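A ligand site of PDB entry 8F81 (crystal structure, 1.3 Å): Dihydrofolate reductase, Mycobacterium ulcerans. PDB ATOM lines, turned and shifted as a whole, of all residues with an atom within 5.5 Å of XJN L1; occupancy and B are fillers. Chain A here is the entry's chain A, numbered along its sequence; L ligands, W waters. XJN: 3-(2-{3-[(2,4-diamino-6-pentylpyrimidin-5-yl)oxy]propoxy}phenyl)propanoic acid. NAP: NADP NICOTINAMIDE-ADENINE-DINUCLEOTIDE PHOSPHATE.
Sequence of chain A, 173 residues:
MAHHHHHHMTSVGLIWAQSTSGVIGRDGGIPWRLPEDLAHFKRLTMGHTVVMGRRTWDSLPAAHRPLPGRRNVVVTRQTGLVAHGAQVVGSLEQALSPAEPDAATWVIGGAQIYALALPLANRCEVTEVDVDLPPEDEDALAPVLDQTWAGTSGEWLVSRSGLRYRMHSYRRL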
ATOM      1  N   ILE A  15       4.736 -23.285 -15.565  1.00  0.00           N
ATOM      2  CA  ILE A  15       3.704 -23.095 -16.577  1.00  0.00           C
ATOM      3  C   ILE A  15       2.347 -23.213 -15.886  1.00  0.00           C
ATOM      4  O   ILE A  15       2.128 -24.166 -15.122  1.00  0.00           O
ATOM      5  CB  ILE A  15       3.869 -24.078 -17.751  1.00  0.00           C
ATOM      6  CG1 ILE A  15       2.827 -23.803 -18.838  1.00  0.00           C
ATOM      7  CG2 ILE A  15       3.873 -25.540 -17.295  1.00  0.00           C
ATOM      8  CD1 ILE A  15       3.150 -24.477 -20.136  1.00  0.00           C
ATOM      9  N   TRP A  16       1.471 -22.226 -16.103  1.00  0.00           N
ATOM     10  CA  TRP A  16       0.146 -22.247 -15.499  1.00  0.00           C
ATOM     11  C   TRP A  16      -0.837 -21.435 -16.332  1.00  0.00           C
ATOM     12  O   TRP A  16      -0.436 -20.617 -17.164  1.00  0.00           O
ATOM     13  CB  TRP A  16       0.145 -21.716 -14.044  1.00  0.00           C
ATOM     14  CG  TRP A  16       0.282 -20.214 -13.833  1.00  0.00           C
ATOM     15  CD1 TRP A  16      -0.726 -19.294 -13.842  1.00  0.00           C
ATOM     16  CD2 TRP A  16       1.491 -19.495 -13.507  1.00  0.00           C
ATOM     17  NE1 TRP A  16      -0.232 -18.035 -13.561  1.00  0.00           N
ATOM     18  CE2 TRP A  16       1.122 -18.135 -13.349  1.00  0.00           C
ATOM     19  CE3 TRP A  16       2.825 -19.845 -13.349  1.00  0.00           C
ATOM     20  CZ2 TRP A  16       2.048 -17.148 -13.039  1.00  0.00           C
ATOM     21  CZ3 TRP A  16       3.751 -18.858 -13.039  1.00  0.00           C
ATOM     22  CH2 TRP A  16       3.353 -17.520 -12.885  1.00  0.00           C
ATOM     23  N   ALA A  17      -2.125 -21.696 -16.098  1.00  0.00           N
ATOM     24  CA  ALA A  17      -3.223 -20.892 -16.639  1.00  0.00           C
ATOM     25  C   ALA A  17      -3.999 -20.276 -15.483  1.00  0.00           C
ATOM     26  O   ALA A  17      -4.229 -20.916 -14.460  1.00  0.00           O
ATOM     27  CB  ALA A  17      -4.139 -21.776 -17.490  1.00  0.00           C
ATOM     28  N   ILE A  30      -9.918 -27.024 -12.141  1.00  0.00           N
ATOM     29  CA  ILE A  30      -9.719 -25.736 -12.791  1.00  0.00           C
ATOM     30  C   ILE A  30     -11.092 -25.191 -13.175  1.00  0.00           C
ATOM     31  O   ILE A  30     -11.849 -25.869 -13.889  1.00  0.00           O
ATOM     32  CB  ILE A  30      -8.796 -25.868 -14.011  1.00  0.00           C
ATOM     33  CG1 ILE A  30      -7.412 -26.339 -13.575  1.00  0.00           C
ATOM     34  CG2 ILE A  30      -8.658 -24.558 -14.730  1.00  0.00           C
ATOM     35  CD1 ILE A  30      -6.489 -26.720 -14.707  1.00  0.00           C
ATOM     36  N   ARG A  33     -12.948 -24.070 -18.771  1.00  0.00           N
ATOM     37  CA  ARG A  33     -12.482 -24.999 -19.790  1.00  0.00           C
ATOM     38  C   ARG A  33     -11.986 -24.209 -20.978  1.00  0.00           C
ATOM     39  O   ARG A  33     -12.717 -23.389 -21.542  1.00  0.00           O
ATOM     40  CB  ARG A  33     -13.593 -25.972 -20.220  1.00  0.00           C
ATOM     41  CG  ARG A  33     -13.187 -26.865 -21.386  1.00  0.00           C
ATOM     42  CD  ARG A  33     -14.132 -28.058 -21.555  1.00  0.00           C
ATOM     43  NE  ARG A  33     -13.898 -28.764 -22.800  1.00  0.00           N
ATOM     44  CZ  ARG A  33     -12.941 -29.670 -22.994  1.00  0.00           C
ATOM     45  NH1 ARG A  33     -12.114 -30.006 -22.022  1.00  0.00           N
ATOM     46  NH2 ARG A  33     -12.826 -30.234 -24.190  1.00  0.00           N
ATOM     47  N   LEU A  34     -10.725 -24.442 -21.347  1.00  0.00           N
ATOM     48  CA  LEU A  34     -10.092 -23.708 -22.433  1.00  0.00           C
ATOM     49  C   LEU A  34      -9.264 -24.695 -23.244  1.00  0.00           C
ATOM     50  O   LEU A  34      -8.070 -24.893 -22.964  1.00  0.00           O
ATOM     51  CB  LEU A  34      -9.262 -22.549 -21.899  1.00  0.00           C
ATOM     52  CG  LEU A  34      -8.642 -21.657 -22.975  1.00  0.00           C
ATOM     53  CD1 LEU A  34      -9.690 -21.103 -23.901  1.00  0.00           C
ATOM     54  CD2 LEU A  34      -7.861 -20.539 -22.319  1.00  0.00           C
ATOM     55  N   ASP A  37      -5.783 -23.762 -24.379  1.00  0.00           N
ATOM     56  CA  ASP A  37      -4.732 -23.805 -23.369  1.00  0.00           C
ATOM     57  C   ASP A  37      -4.189 -25.220 -23.197  1.00  0.00           C
ATOM     58  O   ASP A  37      -2.985 -25.405 -22.994  1.00  0.00           O
ATOM     59  CB  ASP A  37      -5.229 -23.241 -22.045  1.00  0.00           C
ATOM     60  CG  ASP A  37      -4.209 -23.422 -20.958  1.00  0.00           C
ATOM     61  OD1 ASP A  37      -3.118 -22.806 -21.047  1.00  0.00           O
ATOM     62  OD2 ASP A  37      -4.483 -24.207 -20.032  1.00  0.00           O
ATOM     63  N   LEU A  38      -5.054 -26.229 -23.239  1.00  0.00           N
ATOM     64  CA  LEU A  38      -4.559 -27.601 -23.159  1.00  0.00           C
ATOM     65  C   LEU A  38      -3.595 -27.911 -24.302  1.00  0.00           C
ATOM     66  O   LEU A  38      -2.542 -28.525 -24.079  1.00  0.00           O
ATOM     67  CB  LEU A  38      -5.719 -28.592 -23.128  1.00  0.00           C
ATOM     68  CG  LEU A  38      -5.339 -30.064 -23.217  1.00  0.00           C
ATOM     69  CD1 LEU A  38      -4.335 -30.456 -22.137  1.00  0.00           C
ATOM     70  CD2 LEU A  38      -6.594 -30.901 -23.093  1.00  0.00           C
ATOM     71  N   HIS A  40      -1.737 -25.746 -25.950  1.00  0.00           N
ATOM     72  CA  HIS A  40      -0.533 -24.998 -25.655  1.00  0.00           C
ATOM     73  C   HIS A  40       0.317 -25.724 -24.612  1.00  0.00           C
ATOM     74  O   HIS A  40       1.535 -25.875 -24.767  1.00  0.00           O
ATOM     75  CB  HIS A  40      -0.978 -23.618 -25.134  1.00  0.00           C
ATOM     76  CG  HIS A  40       0.119 -22.783 -24.543  1.00  0.00           C
ATOM     77  ND1 HIS A  40       1.109 -22.212 -25.301  1.00  0.00           N
ATOM     78  CD2 HIS A  40       0.319 -22.363 -23.271  1.00  0.00           C
ATOM     79  CE1 HIS A  40       1.905 -21.507 -24.516  1.00  0.00           C
ATOM     80  NE2 HIS A  40       1.445 -21.585 -23.275  1.00  0.00           N
ATOM     81  N   PHE A  41      -0.334 -26.209 -23.559  1.00  0.00           N
ATOM     82  CA  PHE A  41       0.369 -26.900 -22.477  1.00  0.00           C
ATOM     83  C   PHE A  41       1.043 -28.176 -22.988  1.00  0.00           C
ATOM     84  O   PHE A  41       2.201 -28.444 -22.673  1.00  0.00           O
ATOM     85  CB  PHE A  41      -0.625 -27.224 -21.373  1.00  0.00           C
ATOM     86  CG  PHE A  41      -0.064 -28.071 -20.280  1.00  0.00           C
ATOM     87  CD1 PHE A  41       0.790 -27.522 -19.335  1.00  0.00           C
ATOM     88  CD2 PHE A  41      -0.403 -29.408 -20.174  1.00  0.00           C
ATOM     89  CE1 PHE A  41       1.321 -28.298 -18.324  1.00  0.00           C
ATOM     90  CE2 PHE A  41       0.116 -30.197 -19.146  1.00  0.00           C
ATOM     91  CZ  PHE A  41       0.974 -29.627 -18.224  1.00  0.00           C
ATOM     92  N   LYS A  42       0.324 -28.942 -23.808  1.00  0.00           N
ATOM     93  CA  LYS A  42       0.919 -30.143 -24.399  1.00  0.00           C
ATOM     94  C   LYS A  42       2.103 -29.805 -25.294  1.00  0.00           C
ATOM     95  O   LYS A  42       3.149 -30.470 -25.219  1.00  0.00           O
ATOM     96  CB  LYS A  42      -0.135 -30.881 -25.217  1.00  0.00           C
ATOM     97  CG  LYS A  42      -1.173 -31.659 -24.461  1.00  0.00           C
ATOM     98  CD  LYS A  42      -2.041 -32.359 -25.507  1.00  0.00           C
ATOM     99  CE  LYS A  42      -3.195 -33.120 -24.920  1.00  0.00           C
ATOM    100  NZ  LYS A  42      -4.075 -33.547 -26.035  1.00  0.00           N
ATOM    101  N   THR A  45       5.138 -28.945 -23.137  1.00  0.00           N
ATOM    102  CA  THR A  45       5.652 -29.937 -22.200  1.00  0.00           C
ATOM    103  C   THR A  45       5.960 -31.297 -22.825  1.00  0.00           C
ATOM    104  O   THR A  45       6.649 -32.102 -22.182  1.00  0.00           O
ATOM    105  CB  THR A  45       4.698 -30.154 -21.025  1.00  0.00           C
ATOM    106  OG1 THR A  45       3.424 -30.603 -21.474  1.00  0.00           O
ATOM    107  CG2 THR A  45       4.539 -28.888 -20.181  1.00  0.00           C
ATOM    108  N   THR A  56      -2.431 -31.894  -7.330  1.00  0.00           N
ATOM    109  CA  THR A  56      -2.617 -31.806  -8.782  1.00  0.00           C
ATOM    110  C   THR A  56      -2.621 -33.192  -9.416  1.00  0.00           C
ATOM    111  O   THR A  56      -3.450 -33.486 -10.275  1.00  0.00           O
ATOM    112  CB  THR A  56      -1.543 -30.884  -9.384  1.00  0.00           C
ATOM    113  OG1 THR A  56      -1.758 -29.548  -8.907  1.00  0.00           O
ATOM    114  CG2 THR A  56      -1.596 -30.881 -10.906  1.00  0.00           C
ATOM    115  N   SER A  59      -5.850 -34.660  -8.910  1.00  0.00           N
ATOM    116  CA  SER A  59      -6.880 -33.908  -9.633  1.00  0.00           C
ATOM    117  C   SER A  59      -7.022 -34.354 -11.080  1.00  0.00           C
ATOM    118  O   SER A  59      -8.054 -34.075 -11.699  1.00  0.00           O
ATOM    119  CB  SER A  59      -6.575 -32.405  -9.596  1.00  0.00           C
ATOM    120  OG  SER A  59      -5.647 -32.034 -10.609  1.00  0.00           O
ATOM    121  N   LEU A  60      -6.023 -35.019 -11.632  1.00  0.00           N
ATOM    122  CA  LEU A  60      -6.038 -35.347 -13.059  1.00  0.00           C
ATOM    123  C   LEU A  60      -7.150 -36.350 -13.342  1.00  0.00           C
ATOM    124  O   LEU A  60      -7.281 -37.346 -12.620  1.00  0.00           O
ATOM    125  CB  LEU A  60      -4.696 -35.937 -13.474  1.00  0.00           C
ATOM    126  CG  LEU A  60      -3.503 -34.987 -13.392  1.00  0.00           C
ATOM    127  CD1 LEU A  60      -2.193 -35.741 -13.715  1.00  0.00           C
ATOM    128  CD2 LEU A  60      -3.688 -33.788 -14.307  1.00  0.00           C
ATOM    129  N   PRO A  61      -7.981 -36.115 -14.349  1.00  0.00           N
ATOM    130  CA  PRO A  61      -8.905 -37.161 -14.800  1.00  0.00           C
ATOM    131  C   PRO A  61      -8.125 -38.399 -15.212  1.00  0.00           C
ATOM    132  O   PRO A  61      -6.977 -38.305 -15.652  1.00  0.00           O
ATOM    133  CB  PRO A  61      -9.597 -36.523 -16.013  1.00  0.00           C
ATOM    134  CG  PRO A  61      -9.472 -35.056 -15.783  1.00  0.00           C
ATOM    135  CD  PRO A  61      -8.150 -34.861 -15.106  1.00  0.00           C
ATOM    136  N   HIS A  64      -6.015 -38.716 -18.248  1.00  0.00           N
ATOM    137  CA  HIS A  64      -4.853 -37.828 -18.358  1.00  0.00           C
ATOM    138  C   HIS A  64      -3.823 -38.084 -17.260  1.00  0.00           C
ATOM    139  O   HIS A  64      -2.941 -37.248 -17.055  1.00  0.00           O
ATOM    140  CB  HIS A  64      -5.326 -36.369 -18.322  1.00  0.00           C
ATOM    141  CG  HIS A  64      -6.297 -36.032 -19.412  1.00  0.00           C
ATOM    142  ND1 HIS A  64      -5.926 -35.914 -20.737  1.00  0.00           N
ATOM    143  CD2 HIS A  64      -7.630 -35.798 -19.371  1.00  0.00           C
ATOM    144  CE1 HIS A  64      -6.993 -35.624 -21.462  1.00  0.00           C
ATOM    145  NE2 HIS A  64      -8.034 -35.543 -20.664  1.00  0.00           N
ATOM    146  N   LEU A  67       0.246 -37.865 -17.366  1.00  0.00           N
ATOM    147  CA  LEU A  67       0.202 -37.090 -18.593  1.00  0.00           C
ATOM    148  C   LEU A  67       1.014 -37.842 -19.640  1.00  0.00           C
ATOM    149  O   LEU A  67       2.219 -38.049 -19.434  1.00  0.00           O
ATOM    150  CB  LEU A  67       0.817 -35.728 -18.319  1.00  0.00           C
ATOM    151  CG  LEU A  67       0.041 -34.885 -17.309  1.00  0.00           C
ATOM    152  CD1 LEU A  67       0.811 -33.619 -17.059  1.00  0.00           C
ATOM    153  CD2 LEU A  67      -1.354 -34.583 -17.799  1.00  0.00           C
ATOM    154  N   PRO A  68       0.406 -38.272 -20.746  1.00  0.00           N
ATOM    155  CA  PRO A  68       1.131 -39.138 -21.680  1.00  0.00           C
ATOM    156  C   PRO A  68       2.270 -38.401 -22.372  1.00  0.00           C
ATOM    157  O   PRO A  68       2.191 -37.200 -22.650  1.00  0.00           O
ATOM    158  CB  PRO A  68       0.051 -39.552 -22.682  1.00  0.00           C
ATOM    159  CG  PRO A  68      -0.936 -38.441 -22.637  1.00  0.00           C
ATOM    160  CD  PRO A  68      -0.966 -38.004 -21.189  1.00  0.00           C
ATOM    161  N   ARG A  70       5.157 -37.658 -21.236  1.00  0.00           N
ATOM    162  CA  ARG A  70       5.954 -36.846 -20.327  1.00  0.00           C
ATOM    163  C   ARG A  70       6.326 -37.686 -19.127  1.00  0.00           C
ATOM    164  O   ARG A  70       5.607 -38.596 -18.735  1.00  0.00           O
ATOM    165  CB  ARG A  70       5.150 -35.628 -19.895  1.00  0.00           C
ATOM    166  CG  ARG A  70       5.143 -34.589 -20.980  1.00  0.00           C
ATOM    167  CD  ARG A  70       3.880 -33.788 -21.030  1.00  0.00           C
ATOM    168  NE  ARG A  70       2.738 -34.554 -21.528  1.00  0.00           N
ATOM    169  CZ  ARG A  70       1.506 -34.075 -21.570  1.00  0.00           C
ATOM    170  NH1 ARG A  70       1.249 -32.828 -21.211  1.00  0.00           N
ATOM    171  NH2 ARG A  70       0.509 -34.879 -21.953  1.00  0.00           N
ATOM    172  N   VAL A 107       7.502 -27.181 -14.175  1.00  0.00           N
ATOM    173  CA  VAL A 107       6.721 -27.264 -12.946  1.00  0.00           C
ATOM    174  C   VAL A 107       5.295 -26.860 -13.303  1.00  0.00           C
ATOM    175  O   VAL A 107       5.068 -25.755 -13.805  1.00  0.00           O
ATOM    176  CB  VAL A 107       7.327 -26.386 -11.848  1.00  0.00           C
ATOM    177  CG1 VAL A 107       6.433 -26.366 -10.616  1.00  0.00           C
ATOM    178  CG2 VAL A 107       8.726 -26.881 -11.512  1.00  0.00           C
ATOM    179  N   ILE A 108       4.342 -27.769 -13.101  1.00  0.00           N
ATOM    180  CA  ILE A 108       3.014 -27.635 -13.692  1.00  0.00           C
ATOM    181  C   ILE A 108       1.915 -27.444 -12.652  1.00  0.00           C
ATOM    182  O   ILE A 108       0.724 -27.564 -13.001  1.00  0.00           O
ATOM    183  CB  ILE A 108       2.692 -28.801 -14.647  1.00  0.00           C
ATOM    184  CG1 ILE A 108       2.512 -30.097 -13.849  1.00  0.00           C
ATOM    185  CG2 ILE A 108       3.777 -28.923 -15.730  1.00  0.00           C
ATOM    186  CD1 ILE A 108       1.856 -31.181 -14.669  1.00  0.00           C
ATOM    187  N   GLY A 109       2.281 -27.147 -11.410  1.00  0.00           N
ATOM    188  CA  GLY A 109       1.339 -26.793 -10.348  1.00  0.00           C
ATOM    189  C   GLY A 109       1.266 -27.864  -9.268  1.00  0.00           C
ATOM    190  O   GLY A 109       1.902 -28.905  -9.338  1.00  0.00           O
ATOM    191  N   TYR A 114       4.165 -24.372  -7.026  1.00  0.00           N
ATOM    192  CA  TYR A 114       4.672 -23.136  -7.643  1.00  0.00           C
ATOM    193  C   TYR A 114       5.455 -22.305  -6.641  1.00  0.00           C
ATOM    194  O   TYR A 114       6.510 -21.763  -6.962  1.00  0.00           O
ATOM    195  CB  TYR A 114       3.551 -22.269  -8.237  1.00  0.00           C
ATOM    196  CG  TYR A 114       2.861 -22.842  -9.460  1.00  0.00           C
ATOM    197  CD1 TYR A 114       3.578 -23.440 -10.494  1.00  0.00           C
ATOM    198  CD2 TYR A 114       1.473 -22.758  -9.585  1.00  0.00           C
ATOM    199  CE1 TYR A 114       2.924 -23.962 -11.624  1.00  0.00           C
ATOM    200  CE2 TYR A 114       0.824 -23.296 -10.681  1.00  0.00           C
ATOM    201  CZ  TYR A 114       1.549 -23.875 -11.702  1.00  0.00           C
ATOM    202  OH  TYR A 114       0.876 -24.420 -12.774  1.00  0.00           O
ATOM    203  N   GLU A 125       5.607 -19.449 -18.063  1.00  0.00           N
ATOM    204  CA  GLU A 125       4.731 -19.431 -19.231  1.00  0.00           C
ATOM    205  C   GLU A 125       3.297 -19.412 -18.714  1.00  0.00           C
ATOM    206  O   GLU A 125       2.841 -20.394 -18.111  1.00  0.00           O
ATOM    207  CB  GLU A 125       4.986 -20.637 -20.118  1.00  0.00           C
ATOM    208  CG  GLU A 125       6.343 -20.631 -20.801  1.00  0.00           C
ATOM    209  CD  GLU A 125       6.499 -19.462 -21.762  1.00  0.00           C
ATOM    210  OE1 GLU A 125       5.478 -18.894 -22.199  1.00  0.00           O
ATOM    211  OE2 GLU A 125       7.652 -19.098 -22.056  1.00  0.00           O
ATOM    212  N   THR A 127      -0.866 -18.630 -19.252  1.00  0.00           N
ATOM    213  CA  THR A 127      -2.064 -18.353 -20.037  1.00  0.00           C
ATOM    214  C   THR A 127      -3.013 -17.558 -19.154  1.00  0.00           C
ATOM    215  O   THR A 127      -3.377 -17.996 -18.061  1.00  0.00           O
ATOM    216  CB  THR A 127      -2.725 -19.645 -20.477  1.00  0.00           C
ATOM    217  OG1 THR A 127      -1.790 -20.452 -21.202  1.00  0.00           O
ATOM    218  CG2 THR A 127      -3.939 -19.335 -21.366  1.00  0.00           C
HETATM  219  C1  XJN L   1      -1.386 -24.585 -18.282  1.00  0.00           C
HETATM  220  C3  XJN L   1      -1.962 -26.559 -16.570  1.00  0.00           C
HETATM  221  N4  XJN L   1      -2.592 -25.167 -18.372  1.00  0.00           N
HETATM  222  O2  XJN L   1      -3.626 -30.912 -16.492  1.00  0.00           O
HETATM  223  O3  XJN L   1      -2.177 -34.243 -21.681  1.00  0.00           O
HETATM  224  C4  XJN L   1      -1.529 -28.841 -15.891  1.00  0.00           C
HETATM  225  N3  XJN L   1       0.257 -26.212 -15.609  1.00  0.00           N
HETATM  226  C2  XJN L   1      -0.686 -25.883 -16.549  1.00  0.00           C
HETATM  227  N2  XJN L   1      -0.425 -24.891 -17.400  1.00  0.00           N
HETATM  228  N1  XJN L   1      -1.111 -23.594 -19.154  1.00  0.00           N
HETATM  229  C8  XJN L   1      -5.970 -31.369 -16.141  1.00  0.00           C
HETATM  230  C5  XJN L   1      -2.113 -29.886 -14.976  1.00  0.00           C
HETATM  231  C6  XJN L   1      -3.559 -30.233 -15.231  1.00  0.00           C
HETATM  232  C10 XJN L   1      -7.171 -32.538 -17.841  1.00  0.00           C
HETATM  233  C11 XJN L   1      -6.022 -32.599 -18.610  1.00  0.00           C
HETATM  234  C12 XJN L   1      -4.810 -32.065 -18.163  1.00  0.00           C
HETATM  235  C13 XJN L   1      -3.550 -32.132 -19.006  1.00  0.00           C
HETATM  236  C14 XJN L   1      -3.574 -33.237 -20.056  1.00  0.00           C
HETATM  237  C15 XJN L   1      -2.304 -33.290 -20.893  1.00  0.00           C
HETATM  238  C16 XJN L   1      -2.885 -26.163 -17.511  1.00  0.00           C
HETATM  239  C17 XJN L   1      -4.233 -26.802 -17.659  1.00  0.00           C
HETATM  240  C18 XJN L   1      -4.289 -27.674 -18.911  1.00  0.00           C
HETATM  241  C19 XJN L   1      -5.455 -28.653 -19.041  1.00  0.00           C
HETATM  242  C20 XJN L   1      -6.821 -28.021 -18.936  1.00  0.00           C
HETATM  243  C21 XJN L   1      -7.923 -29.042 -19.148  1.00  0.00           C
HETATM  244  C7  XJN L   1      -4.813 -31.440 -16.904  1.00  0.00           C
HETATM  245  C9  XJN L   1      -7.138 -31.923 -16.617  1.00  0.00           C
HETATM  246  O1  XJN L   1      -2.235 -27.599 -15.704  1.00  0.00           O
HETATM  247  O4  XJN L   1      -1.451 -32.382 -20.770  1.00  0.00           O
HETATM  248  PA  NAP L   2      -0.426 -28.886  -5.104  1.00  0.00           P
HETATM  249  O1A NAP L   2       0.668 -27.887  -5.032  1.00  0.00           O
HETATM  250  O2A NAP L   2      -0.757 -29.488  -6.429  1.00  0.00           O
HETATM  251  O5B NAP L   2      -0.086 -30.113  -4.137  1.00  0.00           O
HETATM  252  C5B NAP L   2       0.082 -29.938  -2.714  1.00  0.00           C
HETATM  253  C4B NAP L   2       0.730 -31.186  -2.179  1.00  0.00           C
HETATM  254  O4B NAP L   2       2.117 -31.242  -2.587  1.00  0.00           O
HETATM  255  C3B NAP L   2       0.784 -31.335  -0.652  1.00  0.00           C
HETATM  256  O3B NAP L   2      -0.481 -31.744  -0.150  1.00  0.00           O
HETATM  257  C2B NAP L   2       1.905 -32.363  -0.513  1.00  0.00           C
HETATM  258  O2B NAP L   2       1.513 -33.672  -0.925  1.00  0.00           O
HETATM  259  C1B NAP L   2       2.880 -31.861  -1.573  1.00  0.00           C
HETATM  260  N9A NAP L   2       3.855 -30.919  -1.053  1.00  0.00           N
HETATM  261  C8A NAP L   2       3.708 -29.563  -0.893  1.00  0.00           C
HETATM  262  N7A NAP L   2       4.782 -28.981  -0.402  1.00  0.00           N
HETATM  263  C5A NAP L   2       5.686 -30.011  -0.238  1.00  0.00           C
HETATM  264  C6A NAP L   2       7.011 -30.049   0.238  1.00  0.00           C
HETATM  265  N6A NAP L   2       7.677 -28.978   0.657  1.00  0.00           N
HETATM  266  N1A NAP L   2       7.633 -31.249   0.271  1.00  0.00           N
HETATM  267  C2A NAP L   2       6.967 -32.334  -0.152  1.00  0.00           C
HETATM  268  N3A NAP L   2       5.723 -32.420  -0.611  1.00  0.00           N
HETATM  269  C4A NAP L   2       5.131 -31.212  -0.645  1.00  0.00           C
HETATM  270  O3  NAP L   2      -1.752 -28.352  -4.384  1.00  0.00           O
HETATM  271  PN  NAP L   2      -2.597 -27.000  -4.425  1.00  0.00           P
HETATM  272  O1N NAP L   2      -1.705 -25.850  -4.099  1.00  0.00           O
HETATM  273  O2N NAP L   2      -3.822 -27.234  -3.598  1.00  0.00           O
HETATM  274  O5D NAP L   2      -2.981 -26.896  -5.977  1.00  0.00           O
HETATM  275  C5D NAP L   2      -3.996 -27.772  -6.508  1.00  0.00           C
HETATM  276  C4D NAP L   2      -5.013 -26.941  -7.252  1.00  0.00           C
HETATM  277  O4D NAP L   2      -4.358 -26.262  -8.349  1.00  0.00           O
HETATM  278  C3D NAP L   2      -6.163 -27.735  -7.899  1.00  0.00           C
HETATM  279  O3D NAP L   2      -7.329 -26.915  -7.922  1.00  0.00           O
HETATM  280  C2D NAP L   2      -5.652 -27.934  -9.332  1.00  0.00           C
HETATM  281  O2D NAP L   2      -6.705 -28.194 -10.244  1.00  0.00           O
HETATM  282  C1D NAP L   2      -5.054 -26.555  -9.550  1.00  0.00           C
HETATM  283  N1N NAP L   2      -4.089 -26.451 -10.658  1.00  0.00           N
HETATM  284  C2N NAP L   2      -4.230 -25.450 -11.589  1.00  0.00           C
HETATM  285  C3N NAP L   2      -3.298 -25.318 -12.612  1.00  0.00           C
HETATM  286  C7N NAP L   2      -3.469 -24.227 -13.613  1.00  0.00           C
HETATM  287  O7N NAP L   2      -2.586 -24.006 -14.450  1.00  0.00           O
HETATM  288  N7N NAP L   2      -4.593 -23.515 -13.576  1.00  0.00           N
HETATM  289  C4N NAP L   2      -2.229 -26.202 -12.673  1.00  0.00           C
HETATM  290  C5N NAP L   2      -2.091 -27.192 -11.725  1.00  0.00           C
HETATM  291  C6N NAP L   2      -3.012 -27.316 -10.705  1.00  0.00           C
HETATM  292  P2B NAP L   2       1.074 -34.706   0.228  1.00  0.00           P
HETATM  293  O1X NAP L   2       0.844 -35.961  -0.589  1.00  0.00           O
HETATM  294  O2X NAP L   2       2.235 -34.833   1.188  1.00  0.00           O
HETATM  295  O3X NAP L   2      -0.189 -34.147   0.861  1.00  0.00           O
HETATM  296  O   HOH W   1       0.734 -21.388 -20.114  1.00  0.00           O
HETATM  297  O   HOH W   2      -9.593 -28.309 -22.129  1.00  0.00           O
HETATM  298  O   HOH W   3     -10.291 -27.257 -17.631  1.00  0.00           O
HETATM  299  O   HOH W   4      -3.581 -36.247 -21.851  1.00  0.00           O
HETATM  300  O   HOH W   5      -9.024 -26.040 -19.995  1.00  0.00           O
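The backbone NH (N) of Trp 16 sits at hydrogen-bond distance from the backbone carbonyl oxygen (O) of Glu 125.
The side-chain hydroxyl (OG1) of Thr 45 sits at hydrogen-bond distance from the guanidinium group (NH1) of Arg 70.
The guanidinium group (NE) of Arg 70 sits at hydrogen-bond distance from the backbone carbonyl oxygen (O) of Pro 68.
OH of Tyr 114 lies close to N of Gly 109, at 3.4 Å.
OG1 of Thr 127 lies within hydrogen-bond range of OD1 of Asp 37 (2.7 Å).
OG1 of Thr 45 sits at hydrogen-bond distance from O of Phe 41 (2.8 Å).
The backbone carbonyl oxygen (O) of Ile 108 is in hydrogen-bond range of the side-chain hydroxyl (OH) of Tyr 114.
The backbone NH (N) of Thr 127 lies within hydrogen-bond range of the backbone carbonyl oxygen (O) of Trp 16.
A nitrogen (N3) of XJN L1 lies within hydrogen-bond range of the backbone carbonyl oxygen (O) of Ile 15 (2.8 Å).
O of Ile 108 lies within hydrogen-bond range of N3 of XJN L1 (3.0 Å).
N3 of XJN L1 sits at hydrogen-bond distance from OH of Tyr 114 (3.4 Å).
An oxygen (O2A) of NAP L2 is in hydrogen-bond range of the side-chain hydroxyl (OG1) of Thr 56 (2.7 Å).
NH1 of Arg 70 is in salt-bridge range of O4 of XJN L1.
The backbone carbonyl oxygen of Ala 17 lies within hydrogen-bond range of a nitrogen (N7N) of NAP L2, 2.8 Å away.
The backbone NH (N) of Thr 56 sits at hydrogen-bond distance from an oxygen (O2A) of NAP L2 (3.1 Å).
OD2 of Asp 37 sits at hydrogen-bond distance from N4 of XJN L1, at 2.7 Å.
The backbone NH (N) of Ala 17 sits at hydrogen-bond distance from an oxygen (O7N) of NAP L2.
Residues that only touch XJN L1: Trp 16 (3.3 Å), Ala 17 (3.7 Å), Ile 30 (3.7 Å), Leu 38 (3.6 Å), Phe 41 (3.1 Å), Lys 42 (3.6 Å), Leu 60 (3.6 Å), Pro 61 (3.5 Å), His 64 (3.5 Å), Leu 67 (3.4 Å), Pro 68 (3.98 Å) and Thr 127 (3.8 Å).
Hydrophobic or aromatic side chains within 4 Å of XJN L1: Ile 15, Ala 17, Ile 30, Leu 38, Phe 41, Leu 60, Pro 61, His 64, Leu 67, Pro 68 and Ile 108.
The nearest printed residue that does not touch XJN L1 is Thr 56 (4.2 Å).
Water W4 bridges O3 of XJN L1 and ND1 of His 64.
Water W1 lies within hydrogen-bond range of the side-chain hydroxyl (OG1) of Thr 127 (2.9 Å), a nitrogen (N1) of XJN L1 (3.0 Å), the backbone carbonyl oxygen (O) of Glu 125 (3.1 Å), a ring nitrogen (NE2) of His 40 (3.2 Å) and the backbone carbonyl oxygen (O) of Trp 16 (3.3 Å).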
